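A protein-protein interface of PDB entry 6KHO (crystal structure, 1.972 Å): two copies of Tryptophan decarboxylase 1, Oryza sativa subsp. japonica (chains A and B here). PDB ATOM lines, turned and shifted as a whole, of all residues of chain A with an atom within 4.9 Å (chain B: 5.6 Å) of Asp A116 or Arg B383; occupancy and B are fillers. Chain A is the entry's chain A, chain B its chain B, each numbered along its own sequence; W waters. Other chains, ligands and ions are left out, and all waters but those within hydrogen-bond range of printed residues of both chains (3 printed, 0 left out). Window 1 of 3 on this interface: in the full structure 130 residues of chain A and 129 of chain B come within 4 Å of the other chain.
NH1 of Arg B383 is in salt-bridge range of OD2 of Asp A116.
The backbone carbonyl oxygen of Leu A336 is in hydrogen-bond range of the guanidinium group of Arg B383, at 2.8 Å.
The side-chain carboxylate (OD1) of Asp A337 lies within hydrogen-bond range of the backbone NH (N) of Arg B383.
NH2 of Arg A383 lies within salt-bridge range of OD1 of Asp A116 (3.4 Å).
The side-chain amino group (NZ) of Lys A388 is in salt-bridge range of the side-chain carboxylate (OD2) of Asp A116.
O of Cys A335 is in hydrogen-bond range of NZ of Lys A388, 2.8 Å away.
The backbone carbonyl oxygen (O) of Asp B116 lies within hydrogen-bond range of the side-chain hydroxyl (OG) of Ser B120, 3.0 Å away.
NH2 of Arg B383 lies within salt-bridge range of OD1 of Asp B116.
The side-chain hydroxyl (OG) of Ser B120 lies within hydrogen-bond range of the guanidinium group (NH1) of Arg B383, 2.8 Å away.
Among the printed residues, pairs that only touch across the chains: Asp A337 with Arg B382 (3.3 Å), Ile A113 with Leu B117 (3.5 Å), Cys A335 with Ser B120 (3.8 Å), Leu A336 with Arg B382 (3.8 Å), Ser A120 with Asp B116 (3.9 Å) and Leu A336 with Gly B381 (3.97 Å).
Of chain A, only Asp A116 (3.6 Å), Leu A336 (2.8 Å) and Asp A337 (2.9 Å) come within 4 Å of Arg B383.
Of the printed residues of chain B, Asp A337 touches Arg B382 and Arg B383.
Of the printed residues of chain A, Leu B117 touches Ile A113.
Of the printed residues of chain B, Leu A336 touches Gly B381, Arg B382 and Arg B383.
Printed residues of chain A within 4 Å of Ser B120: Cys A335 (3.8 Å).
Leu A117 touches none of the printed residues of chain B.
Arg A383 touches none of the printed residues of chain B.
The nearest residue of chain B that does not touch Asp A116 is Ser B120 (4.1 Å).
The nearest printed residue of chain A that does not touch Leu B117 is Leu A117 (4.1 Å).
Hydrophobic or aromatic side chains of chain B that line the printed part of chain A: Leu B117.
Among the printed residues, 9 pairs touch across the chains.
Among the printed residues, Asp or Glu carboxylates within 4 Å of a Lys or Arg side-chain nitrogen of the other chain: Asp A116 with Arg B383 (3.6 Å).
Asp A116 touches Arg B383, but with the chains exchanged Arg A383 does not touch Asp B116 (4.1 Å).
Ser A120 touches Asp B116, but with the chains exchanged Asp A116 does not touch Ser B120 (4.1 Å).
Positions printed for both chains: 115, 116, 117, 119, 120, 383 and 384.
Of the 9 pairs that touch across the chains among the printed residues, none has its exchanged pair printed and touching as well.
Water W2 lies within hydrogen-bond range of NE of Arg B385 (2.7 Å) and OD2 of Asp A337 (2.9 Å).
Water W3 lies within hydrogen-bond range of O of Ile A113, N of Leu A117 and OG of Ser B120.
Water W1 bridges O of Leu A336 (3.4 Å) and NH1 of Arg B383 (3.4 Å).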
ATOM      1  N   ALA A 112      33.211  32.909  -1.786  1.00  0.00           N
ATOM      2  CA  ALA A 112      32.324  32.581  -0.673  1.00  0.00           C
ATOM      3  C   ALA A 112      31.462  31.370  -0.987  1.00  0.00           C
ATOM      4  O   ALA A 112      31.264  30.505  -0.127  1.00  0.00           O
ATOM      5  CB  ALA A 112      31.438  33.777  -0.318  1.00  0.00           C
ATOM      6  N   ILE A 113      30.934  31.298  -2.212  1.00  0.00           N
ATOM      7  CA  ILE A 113      30.158  30.131  -2.625  1.00  0.00           C
ATOM      8  C   ILE A 113      31.030  28.879  -2.609  1.00  0.00           C
ATOM      9  O   ILE A 113      30.604  27.818  -2.139  1.00  0.00           O
ATOM     10  CB  ILE A 113      29.536  30.361  -4.013  1.00  0.00           C
ATOM     11  CG1 ILE A 113      28.552  31.535  -3.962  1.00  0.00           C
ATOM     12  CG2 ILE A 113      28.825  29.107  -4.473  1.00  0.00           C
ATOM     13  CD1 ILE A 113      28.254  32.134  -5.348  1.00  0.00           C
ATOM     14  N   ALA A 114      32.267  28.991  -3.107  1.00  0.00           N
ATOM     15  CA  ALA A 114      33.210  27.876  -3.062  1.00  0.00           C
ATOM     16  C   ALA A 114      33.453  27.421  -1.632  1.00  0.00           C
ATOM     17  O   ALA A 114      33.403  26.220  -1.328  1.00  0.00           O
ATOM     18  CB  ALA A 114      34.534  28.281  -3.723  1.00  0.00           C
ATOM     19  N   GLY A 115      33.690  28.380  -0.728  1.00  0.00           N
ATOM     20  CA  GLY A 115      33.942  28.029   0.657  1.00  0.00           C
ATOM     21  C   GLY A 115      32.752  27.359   1.313  1.00  0.00           C
ATOM     22  O   GLY A 115      32.904  26.376   2.047  1.00  0.00           O
ATOM     23  N   ASP A 116      31.546  27.865   1.047  1.00  0.00           N
ATOM     24  CA  ASP A 116      30.382  27.237   1.656  1.00  0.00           C
ATOM     25  C   ASP A 116      30.104  25.864   1.069  1.00  0.00           C
ATOM     26  O   ASP A 116      29.653  24.970   1.793  1.00  0.00           O
ATOM     27  CB  ASP A 116      29.146  28.117   1.538  1.00  0.00           C
ATOM     28  CG  ASP A 116      28.688  28.623   2.899  1.00  0.00           C
ATOM     29  OD1 ASP A 116      29.437  28.408   3.895  1.00  0.00           O
ATOM     30  OD2 ASP A 116      27.597  29.218   2.989  1.00  0.00           O
ATOM     31  N   LEU A 117      30.365  25.675  -0.223  1.00  0.00           N
ATOM     32  CA  LEU A 117      30.251  24.344  -0.816  1.00  0.00           C
ATOM     33  C   LEU A 117      31.200  23.357  -0.144  1.00  0.00           C
ATOM     34  O   LEU A 117      30.811  22.231   0.197  1.00  0.00           O
ATOM     35  CB  LEU A 117      30.524  24.431  -2.320  1.00  0.00           C
ATOM     36  CG  LEU A 117      30.811  23.171  -3.136  1.00  0.00           C
ATOM     37  CD1 LEU A 117      29.644  22.199  -3.105  1.00  0.00           C
ATOM     38  CD2 LEU A 117      31.161  23.571  -4.576  1.00  0.00           C
ATOM     39  N   ILE A 118      32.450  23.764   0.064  1.00  0.00           N
ATOM     40  CA  ILE A 118      33.407  22.876   0.720  1.00  0.00           C
ATOM     41  C   ILE A 118      32.955  22.561   2.146  1.00  0.00           C
ATOM     42  O   ILE A 118      33.007  21.405   2.588  1.00  0.00           O
ATOM     43  CB  ILE A 118      34.817  23.491   0.654  1.00  0.00           C
ATOM     44  CG1 ILE A 118      35.289  23.468  -0.811  1.00  0.00           C
ATOM     45  CG2 ILE A 118      35.786  22.705   1.529  1.00  0.00           C
ATOM     46  CD1 ILE A 118      36.537  24.311  -1.124  1.00  0.00           C
ATOM     47  N   ALA A 119      32.446  23.565   2.866  1.00  0.00           N
ATOM     48  CA  ALA A 119      31.993  23.319   4.229  1.00  0.00           C
ATOM     49  C   ALA A 119      30.816  22.354   4.250  1.00  0.00           C
ATOM     50  O   ALA A 119      30.750  21.464   5.109  1.00  0.00           O
ATOM     51  CB  ALA A 119      31.634  24.641   4.912  1.00  0.00           C
ATOM     52  N   SER A 120      29.898  22.486   3.283  1.00  0.00           N
ATOM     53  CA  SER A 120      28.738  21.597   3.211  1.00  0.00           C
ATOM     54  C   SER A 120      29.145  20.163   2.928  1.00  0.00           C
ATOM     55  O   SER A 120      28.465  19.229   3.363  1.00  0.00           O
ATOM     56  CB  SER A 120      27.774  22.044   2.105  1.00  0.00           C
ATOM     57  OG  SER A 120      27.146  23.255   2.421  1.00  0.00           O
ATOM     58  N   CYS A 335      27.990  34.832   1.137  1.00  0.00           N
ATOM     59  CA  CYS A 335      26.596  34.402   1.051  1.00  0.00           C
ATOM     60  C   CYS A 335      26.032  34.082   2.442  1.00  0.00           C
ATOM     61  O   CYS A 335      26.766  33.730   3.375  1.00  0.00           O
ATOM     62  CB  CYS A 335      26.467  33.173   0.134  1.00  0.00           C
ATOM     63  SG  CYS A 335      27.463  31.706   0.636  1.00  0.00           S
ATOM     64  N   LEU A 336      24.706  34.198   2.571  1.00  0.00           N
ATOM     65  CA  LEU A 336      24.046  33.871   3.835  1.00  0.00           C
ATOM     66  C   LEU A 336      24.332  32.421   4.234  1.00  0.00           C
ATOM     67  O   LEU A 336      24.535  31.558   3.375  1.00  0.00           O
ATOM     68  CB  LEU A 336      22.532  34.092   3.710  1.00  0.00           C
ATOM     69  CG  LEU A 336      21.981  35.523   3.834  1.00  0.00           C
ATOM     70  CD1 LEU A 336      22.180  36.348   2.562  1.00  0.00           C
ATOM     71  CD2 LEU A 336      20.502  35.478   4.213  1.00  0.00           C
ATOM     72  N   ASP A 337      24.373  32.141   5.546  1.00  0.00           N
ATOM     73  CA  ASP A 337      24.302  33.124   6.645  1.00  0.00           C
ATOM     74  C   ASP A 337      25.698  33.422   7.190  1.00  0.00           C
ATOM     75  O   ASP A 337      26.555  32.526   7.243  1.00  0.00           O
ATOM     76  CB  ASP A 337      23.441  32.618   7.817  1.00  0.00           C
ATOM     77  CG  ASP A 337      22.225  31.816   7.373  1.00  0.00           C
ATOM     78  OD1 ASP A 337      21.421  32.346   6.580  1.00  0.00           O
ATOM     79  OD2 ASP A 337      22.070  30.656   7.822  1.00  0.00           O
ATOM     80  N   ARG A 383      27.709  24.837  11.699  1.00  0.00           N
ATOM     81  CA  ARG A 383      28.457  24.713  10.455  1.00  0.00           C
ATOM     82  C   ARG A 383      29.821  25.390  10.568  1.00  0.00           C
ATOM     83  O   ARG A 383      30.049  26.264  11.403  1.00  0.00           O
ATOM     84  CB  ARG A 383      27.709  25.378   9.289  1.00  0.00           C
ATOM     85  CG  ARG A 383      26.535  24.606   8.739  1.00  0.00           C
ATOM     86  CD  ARG A 383      25.864  25.395   7.597  1.00  0.00           C
ATOM     87  NE  ARG A 383      26.816  25.767   6.549  1.00  0.00           N
ATOM     88  CZ  ARG A 383      27.132  25.002   5.516  1.00  0.00           C
ATOM     89  NH1 ARG A 383      26.575  23.796   5.362  1.00  0.00           N
ATOM     90  NH2 ARG A 383      28.006  25.450   4.625  1.00  0.00           N
ATOM     91  N   PHE A 384      30.716  24.992   9.665  1.00  0.00           N
ATOM     92  CA  PHE A 384      32.031  25.609   9.475  1.00  0.00           C
ATOM     93  C   PHE A 384      31.871  26.892   8.645  1.00  0.00           C
ATOM     94  O   PHE A 384      32.244  26.969   7.474  1.00  0.00           O
ATOM     95  CB  PHE A 384      32.942  24.587   8.800  1.00  0.00           C
ATOM     96  CG  PHE A 384      34.396  24.988   8.699  1.00  0.00           C
ATOM     97  CD1 PHE A 384      34.862  26.194   9.211  1.00  0.00           C
ATOM     98  CD2 PHE A 384      35.292  24.140   8.067  1.00  0.00           C
ATOM     99  CE1 PHE A 384      36.198  26.538   9.099  1.00  0.00           C
ATOM    100  CE2 PHE A 384      36.630  24.475   7.950  1.00  0.00           C
ATOM    101  CZ  PHE A 384      37.082  25.675   8.459  1.00  0.00           C
ATOM    102  N   LYS A 388      34.148  30.186   4.560  1.00  0.00           N
ATOM    103  CA  LYS A 388      33.818  31.089   3.459  1.00  0.00           C
ATOM    104  C   LYS A 388      34.281  32.510   3.752  1.00  0.00           C
ATOM    105  O   LYS A 388      34.733  33.215   2.843  1.00  0.00           O
ATOM    106  CB  LYS A 388      32.317  31.061   3.158  1.00  0.00           C
ATOM    107  CG  LYS A 388      31.421  31.582   4.275  1.00  0.00           C
ATOM    108  CD  LYS A 388      29.956  31.452   3.876  1.00  0.00           C
ATOM    109  CE  LYS A 388      29.041  31.533   5.093  1.00  0.00           C
ATOM    110  NZ  LYS A 388      27.602  31.389   4.694  1.00  0.00           N
ATOM    111  N   GLY B 115      21.938  20.934  -3.632  1.00  0.00           N
ATOM    112  CA  GLY B 115      20.893  21.883  -3.277  1.00  0.00           C
ATOM    113  C   GLY B 115      21.409  23.056  -2.460  1.00  0.00           C
ATOM    114  O   GLY B 115      21.019  24.207  -2.683  1.00  0.00           O
ATOM    115  N   ASP B 116      22.312  22.790  -1.515  1.00  0.00           N
ATOM    116  CA  ASP B 116      22.829  23.904  -0.726  1.00  0.00           C
ATOM    117  C   ASP B 116      23.759  24.795  -1.539  1.00  0.00           C
ATOM    118  O   ASP B 116      23.796  26.010  -1.319  1.00  0.00           O
ATOM    119  CB  ASP B 116      23.528  23.403   0.530  1.00  0.00           C
ATOM    120  CG  ASP B 116      22.783  23.819   1.796  1.00  0.00           C
ATOM    121  OD1 ASP B 116      21.662  24.376   1.670  1.00  0.00           O
ATOM    122  OD2 ASP B 116      23.313  23.612   2.903  1.00  0.00           O
ATOM    123  N   LEU B 117      24.486  24.221  -2.500  1.00  0.00           N
ATOM    124  CA  LEU B 117      25.303  25.024  -3.404  1.00  0.00           C
ATOM    125  C   LEU B 117      24.437  25.945  -4.255  1.00  0.00           C
ATOM    126  O   LEU B 117      24.779  27.112  -4.470  1.00  0.00           O
ATOM    127  CB  LEU B 117      26.139  24.104  -4.300  1.00  0.00           C
ATOM    128  CG  LEU B 117      26.746  24.720  -5.561  1.00  0.00           C
ATOM    129  CD1 LEU B 117      27.705  25.826  -5.183  1.00  0.00           C
ATOM    130  CD2 LEU B 117      27.466  23.660  -6.427  1.00  0.00           C
ATOM    131  N   ALA B 119      21.420  27.008  -3.525  1.00  0.00           N
ATOM    132  CA  ALA B 119      20.833  28.006  -2.635  1.00  0.00           C
ATOM    133  C   ALA B 119      21.822  29.135  -2.347  1.00  0.00           C
ATOM    134  O   ALA B 119      21.444  30.313  -2.344  1.00  0.00           O
ATOM    135  CB  ALA B 119      20.360  27.328  -1.351  1.00  0.00           C
ATOM    136  N   SER B 120      23.102  28.793  -2.133  1.00  0.00           N
ATOM    137  CA  SER B 120      24.132  29.803  -1.879  1.00  0.00           C
ATOM    138  C   SER B 120      24.347  30.707  -3.084  1.00  0.00           C
ATOM    139  O   SER B 120      24.691  31.885  -2.920  1.00  0.00           O
ATOM    140  CB  SER B 120      25.466  29.135  -1.521  1.00  0.00           C
ATOM    141  OG  SER B 120      25.352  28.418  -0.305  1.00  0.00           O
ATOM    142  N   THR B 124      18.998  34.031  -1.921  1.00  0.00           N
ATOM    143  CA  THR B 124      17.785  34.778  -1.634  1.00  0.00           C
ATOM    144  C   THR B 124      17.512  34.783  -0.129  1.00  0.00           C
ATOM    145  O   THR B 124      17.989  33.930   0.624  1.00  0.00           O
ATOM    146  CB  THR B 124      16.577  34.199  -2.384  1.00  0.00           C
ATOM    147  OG1 THR B 124      16.313  32.865  -1.933  1.00  0.00           O
ATOM    148  CG2 THR B 124      16.821  34.188  -3.900  1.00  0.00           C
ATOM    149  N   GLU B 139       9.868  25.459   1.151  1.00  0.00           N
ATOM    150  CA  GLU B 139      10.047  25.063   2.545  1.00  0.00           C
ATOM    151  C   GLU B 139       8.758  24.466   3.094  1.00  0.00           C
ATOM    152  O   GLU B 139       8.777  23.404   3.724  1.00  0.00           O
ATOM    153  CB  GLU B 139      10.526  26.254   3.389  1.00  0.00           C
ATOM    154  CG  GLU B 139      11.906  26.755   2.919  1.00  0.00           C
ATOM    155  CD  GLU B 139      12.839  27.190   4.053  1.00  0.00           C
ATOM    156  OE1 GLU B 139      12.394  27.298   5.217  1.00  0.00           O
ATOM    157  OE2 GLU B 139      14.028  27.443   3.755  1.00  0.00           O
ATOM    158  N   GLY B 381      15.971  37.064   8.551  1.00  0.00           N
ATOM    159  CA  GLY B 381      16.577  36.776   7.280  1.00  0.00           C
ATOM    160  C   GLY B 381      17.649  35.703   7.306  1.00  0.00           C
ATOM    161  O   GLY B 381      18.774  35.954   7.759  1.00  0.00           O
ATOM    162  N   ARG B 382      17.333  34.517   6.778  1.00  0.00           N
ATOM    163  CA  ARG B 382      18.276  33.405   6.736  1.00  0.00           C
ATOM    164  C   ARG B 382      18.142  32.684   5.394  1.00  0.00           C
ATOM    165  O   ARG B 382      17.326  33.051   4.542  1.00  0.00           O
ATOM    166  CB  ARG B 382      18.047  32.451   7.919  1.00  0.00           C
ATOM    167  CG  ARG B 382      16.583  32.082   8.123  1.00  0.00           C
ATOM    168  CD  ARG B 382      16.258  30.732   7.523  1.00  0.00           C
ATOM    169  NE  ARG B 382      14.919  30.281   7.896  1.00  0.00           N
ATOM    170  CZ  ARG B 382      14.235  29.339   7.253  1.00  0.00           C
ATOM    171  NH1 ARG B 382      14.763  28.727   6.187  1.00  0.00           N
ATOM    172  NH2 ARG B 382      13.021  29.005   7.678  1.00  0.00           N
ATOM    173  N   ARG B 383      18.950  31.633   5.226  1.00  0.00           N
ATOM    174  CA  ARG B 383      19.099  30.925   3.960  1.00  0.00           C
ATOM    175  C   ARG B 383      17.821  30.226   3.526  1.00  0.00           C
ATOM    176  O   ARG B 383      16.929  29.936   4.325  1.00  0.00           O
ATOM    177  CB  ARG B 383      20.151  29.822   4.060  1.00  0.00           C
ATOM    178  CG  ARG B 383      21.560  30.235   4.114  1.00  0.00           C
ATOM    179  CD  ARG B 383      22.397  28.996   4.304  1.00  0.00           C
ATOM    180  NE  ARG B 383      22.310  28.114   3.150  1.00  0.00           N
ATOM    181  CZ  ARG B 383      23.119  28.190   2.102  1.00  0.00           C
ATOM    182  NH1 ARG B 383      24.081  29.105   2.070  1.00  0.00           N
ATOM    183  NH2 ARG B 383      22.986  27.335   1.096  1.00  0.00           N
ATOM    184  N   PHE B 384      17.817  29.860   2.244  1.00  0.00           N
ATOM    185  CA  PHE B 384      16.829  28.984   1.613  1.00  0.00           C
ATOM    186  C   PHE B 384      17.177  27.517   1.909  1.00  0.00           C
ATOM    187  O   PHE B 384      17.611  26.748   1.044  1.00  0.00           O
ATOM    188  CB  PHE B 384      16.809  29.300   0.120  1.00  0.00           C
ATOM    189  CG  PHE B 384      15.840  28.492  -0.695  1.00  0.00           C
ATOM    190  CD1 PHE B 384      14.824  27.751  -0.104  1.00  0.00           C
ATOM    191  CD2 PHE B 384      15.934  28.512  -2.072  1.00  0.00           C
ATOM    192  CE1 PHE B 384      13.937  27.028  -0.877  1.00  0.00           C
ATOM    193  CE2 PHE B 384      15.046  27.799  -2.858  1.00  0.00           C
ATOM    194  CZ  PHE B 384      14.047  27.053  -2.259  1.00  0.00           C
ATOM    195  N   ARG B 385      16.921  27.121   3.165  1.00  0.00           N
ATOM    196  CA  ARG B 385      17.223  25.774   3.651  1.00  0.00           C
ATOM    197  C   ARG B 385      16.340  24.685   3.038  1.00  0.00           C
ATOM    198  O   ARG B 385      16.716  23.508   3.075  1.00  0.00           O
ATOM    199  CB  ARG B 385      17.077  25.718   5.180  1.00  0.00           C
ATOM    200  CG  ARG B 385      18.066  26.572   5.991  1.00  0.00           C
ATOM    201  CD  ARG B 385      17.646  26.640   7.483  1.00  0.00           C
ATOM    202  NE  ARG B 385      18.481  27.536   8.290  1.00  0.00           N
ATOM    203  CZ  ARG B 385      18.057  28.201   9.364  1.00  0.00           C
ATOM    204  NH1 ARG B 385      16.794  28.076   9.770  1.00  0.00           N
ATOM    205  NH2 ARG B 385      18.890  29.000  10.037  1.00  0.00           N
ATOM    206  N   GLY B 386      15.164  25.033   2.501  1.00  0.00           N
ATOM    207  CA  GLY B 386      14.246  24.009   2.031  1.00  0.00           C
ATOM    208  C   GLY B 386      14.668  23.329   0.739  1.00  0.00           C
ATOM    209  O   GLY B 386      14.229  22.206   0.477  1.00  0.00           O
HETATM  210  O   HOH W   1      22.410  31.781   0.771  1.00  0.00           O
HETATM  211  O   HOH W   2      21.124  27.897   7.888  1.00  0.00           O
HETATM  212  O   HOH W   3      27.791  26.809  -1.611  1.00  0.00           O
